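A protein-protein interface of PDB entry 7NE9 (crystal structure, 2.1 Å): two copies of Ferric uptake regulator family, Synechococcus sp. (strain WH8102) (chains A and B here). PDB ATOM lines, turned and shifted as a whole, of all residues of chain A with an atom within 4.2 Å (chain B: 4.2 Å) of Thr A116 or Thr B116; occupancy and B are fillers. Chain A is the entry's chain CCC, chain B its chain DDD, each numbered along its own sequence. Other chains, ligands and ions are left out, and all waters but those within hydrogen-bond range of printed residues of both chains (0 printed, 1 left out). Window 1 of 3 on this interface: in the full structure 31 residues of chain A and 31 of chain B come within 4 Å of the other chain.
O of Glu B118 sits at hydrogen-bond distance from N of Thr A116 (2.9 Å).
The backbone NH (N) of Thr B116 sits at hydrogen-bond distance from the backbone carbonyl oxygen (O) of Glu A118.
Among the printed residues, pairs that only touch across the chains: Glu A118 with His B115 (3.2 Å), His A115 with Glu B118 (3.2 Å), Leu A117 with Thr B116 (3.3 Å), Thr A116 with Leu B117 (3.4 Å), Thr A116 with Phe B120 (3.8 Å), Thr A116 with Thr B116 (3.9 Å) and Phe A120 with Thr B116 (3.9 Å).
Printed residues of chain B within 4 Å of His A115: Glu B118.
Thr A116 touches four residues of chain B.
Printed residues of chain B within 4 Å of Leu A117: Thr B116 (3.3 Å).
Of chain A, only Thr A116 (3.9 Å), Leu A117 (3.3 Å), Glu A118 (2.8 Å) and Phe A120 (3.9 Å) come within 4 Å of Thr B116.
Of the printed residues of chain A, Leu B117 touches Thr A116.
Printed residues of chain A within 4 Å of Phe B120: Thr A116 (3.8 Å).
The nearest printed residue of chain B that does not touch Thr A116 is His B115 (7.6 Å).
The nearest printed residue of chain A that does not touch His B115 is Leu A117 (4.5 Å).
Printed residues of chain B that touch a printed residue of chain A: His B115, Thr B116, Leu B117, Glu B118 and Phe B120.
Hydrophobic or aromatic side chains of chain B within 4 Å of the printed part of chain A: His B115, Leu B117 and Phe B120.
Of the 6 printed residues of chain A, 5 touch a printed residue of chain B.
Hydrophobic or aromatic side chains of chain A that line the printed part of chain B: His A115, Leu A117 and Phe A120.
His A115 touches Glu B118, and with the chains exchanged Glu A118 touches His B115.
Thr B116 touches its own counterpart, Thr A116.
Thr A116 touches Glu B118, and with the chains exchanged Glu A118 touches Thr B116.
Thr A116 touches Phe B120, and with the chains exchanged Phe A120 touches Thr B116.
Positions printed for both chains: 115, 116, 117, 118 and 120.
Of the 9 pairs that touch across the chains among the printed residues, 9 have their exchanged pair printed and touching as well.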
ATOM      1  N   CYS A  61       4.382 -14.204  -3.098  1.00  0.00           N
ATOM      2  CA  CYS A  61       4.695 -15.608  -2.800  1.00  0.00           C
ATOM      3  C   CYS A  61       4.842 -15.742  -1.291  1.00  0.00           C
ATOM      4  O   CYS A  61       5.350 -14.821  -0.659  1.00  0.00           O
ATOM      5  CB  CYS A  61       5.970 -16.010  -3.532  1.00  0.00           C
ATOM      6  SG  CYS A  61       6.497 -17.705  -3.179  1.00  0.00           S
ATOM      7  N   HIS A 115       4.002  -6.761   2.221  1.00  0.00           N
ATOM      8  CA  HIS A 115       4.547  -7.526   3.360  1.00  0.00           C
ATOM      9  C   HIS A 115       3.872  -8.899   3.414  1.00  0.00           C
ATOM     10  O   HIS A 115       2.705  -9.055   2.980  1.00  0.00           O
ATOM     11  CB  HIS A 115       4.375  -6.755   4.664  1.00  0.00           C
ATOM     12  CG  HIS A 115       2.952  -6.461   5.001  1.00  0.00           C
ATOM     13  ND1 HIS A 115       2.415  -5.202   4.869  1.00  0.00           N
ATOM     14  CD2 HIS A 115       1.971  -7.259   5.481  1.00  0.00           C
ATOM     15  CE1 HIS A 115       1.142  -5.237   5.232  1.00  0.00           C
ATOM     16  NE2 HIS A 115       0.844  -6.493   5.641  1.00  0.00           N
ATOM     17  N   THR A 116       4.630  -9.847   3.932  1.00  0.00           N
ATOM     18  CA  THR A 116       4.182 -11.184   4.353  1.00  0.00           C
ATOM     19  C   THR A 116       4.186 -11.157   5.876  1.00  0.00           C
ATOM     20  O   THR A 116       5.198 -10.697   6.447  1.00  0.00           O
ATOM     21  CB  THR A 116       5.138 -12.216   3.758  1.00  0.00           C
ATOM     22  OG1 THR A 116       4.760 -12.252   2.378  1.00  0.00           O
ATOM     23  CG2 THR A 116       5.013 -13.594   4.349  1.00  0.00           C
ATOM     24  N   LEU A 117       3.102 -11.598   6.487  1.00  0.00           N
ATOM     25  CA  LEU A 117       3.005 -11.717   7.948  1.00  0.00           C
ATOM     26  C   LEU A 117       2.341 -13.045   8.257  1.00  0.00           C
ATOM     27  O   LEU A 117       1.218 -13.253   7.775  1.00  0.00           O
ATOM     28  CB  LEU A 117       2.179 -10.544   8.481  1.00  0.00           C
ATOM     29  CG  LEU A 117       1.923 -10.576   9.979  1.00  0.00           C
ATOM     30  CD1 LEU A 117       3.195 -10.690  10.799  1.00  0.00           C
ATOM     31  CD2 LEU A 117       1.173  -9.331  10.407  1.00  0.00           C
ATOM     32  N   GLU A 118       3.034 -13.917   8.968  1.00  0.00           N
ATOM     33  CA  GLU A 118       2.526 -15.294   9.215  1.00  0.00           C
ATOM     34  C   GLU A 118       2.781 -15.621  10.676  1.00  0.00           C
ATOM     35  O   GLU A 118       3.896 -15.322  11.144  1.00  0.00           O
ATOM     36  CB  GLU A 118       3.134 -16.286   8.207  1.00  0.00           C
ATOM     37  CG  GLU A 118       2.624 -16.085   6.777  1.00  0.00           C
ATOM     38  CD  GLU A 118       1.101 -16.166   6.606  1.00  0.00           C
ATOM     39  OE1 GLU A 118       0.436 -16.809   7.470  1.00  0.00           O
ATOM     40  OE2 GLU A 118       0.566 -15.591   5.635  1.00  0.00           O
ATOM     41  N   PHE A 120       2.667 -18.575  13.809  1.00  0.00           N
ATOM     42  CA  PHE A 120       2.956 -20.010  14.008  1.00  0.00           C
ATOM     43  C   PHE A 120       2.745 -20.307  15.481  1.00  0.00           C
ATOM     44  O   PHE A 120       3.126 -19.486  16.345  1.00  0.00           O
ATOM     45  CB  PHE A 120       4.371 -20.330  13.522  1.00  0.00           C
ATOM     46  CG  PHE A 120       4.515 -20.079  12.049  1.00  0.00           C
ATOM     47  CD1 PHE A 120       4.034 -21.005  11.127  1.00  0.00           C
ATOM     48  CD2 PHE A 120       5.039 -18.885  11.582  1.00  0.00           C
ATOM     49  CE1 PHE A 120       4.119 -20.754   9.766  1.00  0.00           C
ATOM     50  CE2 PHE A 120       5.145 -18.647  10.217  1.00  0.00           C
ATOM     51  CZ  PHE A 120       4.688 -19.581   9.315  1.00  0.00           C
ATOM     52  N   HIS B 115       6.126 -15.260  14.954  1.00  0.00           N
ATOM     53  CA  HIS B 115       5.667 -14.659  13.689  1.00  0.00           C
ATOM     54  C   HIS B 115       6.883 -14.474  12.791  1.00  0.00           C
ATOM     55  O   HIS B 115       8.011 -14.317  13.265  1.00  0.00           O
ATOM     56  CB  HIS B 115       4.910 -13.346  13.932  1.00  0.00           C
ATOM     57  CG  HIS B 115       5.736 -12.309  14.611  1.00  0.00           C
ATOM     58  ND1 HIS B 115       5.568 -11.998  15.953  1.00  0.00           N
ATOM     59  CD2 HIS B 115       6.747 -11.538  14.150  1.00  0.00           C
ATOM     60  CE1 HIS B 115       6.448 -11.045  16.274  1.00  0.00           C
ATOM     61  NE2 HIS B 115       7.197 -10.753  15.186  1.00  0.00           N
ATOM     62  N   THR B 116       6.608 -14.570  11.511  1.00  0.00           N
ATOM     63  CA  THR B 116       7.488 -14.220  10.395  1.00  0.00           C
ATOM     64  C   THR B 116       6.893 -12.939   9.820  1.00  0.00           C
ATOM     65  O   THR B 116       5.676 -12.899   9.573  1.00  0.00           O
ATOM     66  CB  THR B 116       7.534 -15.387   9.410  1.00  0.00           C
ATOM     67  OG1 THR B 116       8.347 -16.352  10.079  1.00  0.00           O
ATOM     68  CG2 THR B 116       8.159 -15.021   8.089  1.00  0.00           C
ATOM     69  N   LEU B 117       7.728 -11.930   9.651  1.00  0.00           N
ATOM     70  CA  LEU B 117       7.332 -10.635   9.068  1.00  0.00           C
ATOM     71  C   LEU B 117       8.424 -10.266   8.080  1.00  0.00           C
ATOM     72  O   LEU B 117       9.576 -10.221   8.487  1.00  0.00           O
ATOM     73  CB  LEU B 117       7.199  -9.602  10.186  1.00  0.00           C
ATOM     74  CG  LEU B 117       6.997  -8.159   9.705  1.00  0.00           C
ATOM     75  CD1 LEU B 117       5.717  -8.052   8.910  1.00  0.00           C
ATOM     76  CD2 LEU B 117       6.987  -7.185  10.863  1.00  0.00           C
ATOM     77  N   GLU B 118       8.059 -10.101   6.823  1.00  0.00           N
ATOM     78  CA  GLU B 118       9.032  -9.834   5.748  1.00  0.00           C
ATOM     79  C   GLU B 118       8.412  -8.743   4.873  1.00  0.00           C
ATOM     80  O   GLU B 118       7.235  -8.853   4.554  1.00  0.00           O
ATOM     81  CB  GLU B 118       9.398 -11.135   5.024  1.00  0.00           C
ATOM     82  CG  GLU B 118      10.202 -12.123   5.876  1.00  0.00           C
ATOM     83  CD  GLU B 118      11.521 -11.602   6.456  1.00  0.00           C
ATOM     84  OE1 GLU B 118      12.061 -10.647   5.857  1.00  0.00           O
ATOM     85  OE2 GLU B 118      12.002 -12.100   7.539  1.00  0.00           O
ATOM     86  N   PHE B 120       8.756  -6.479   1.211  1.00  0.00           N
ATOM     87  CA  PHE B 120       9.181  -6.672  -0.189  1.00  0.00           C
ATOM     88  C   PHE B 120       9.003  -5.364  -0.950  1.00  0.00           C
ATOM     89  O   PHE B 120       8.033  -4.660  -0.711  1.00  0.00           O
ATOM     90  CB  PHE B 120       8.392  -7.842  -0.786  1.00  0.00           C
ATOM     91  CG  PHE B 120       8.687  -9.134  -0.080  1.00  0.00           C
ATOM     92  CD1 PHE B 120       9.838  -9.845  -0.371  1.00  0.00           C
ATOM     93  CD2 PHE B 120       7.860  -9.603   0.923  1.00  0.00           C
ATOM     94  CE1 PHE B 120      10.139 -11.022   0.296  1.00  0.00           C
ATOM     95  CE2 PHE B 120       8.154 -10.783   1.590  1.00  0.00           C
ATOM     96  CZ  PHE B 120       9.294 -11.485   1.281  1.00  0.00           C
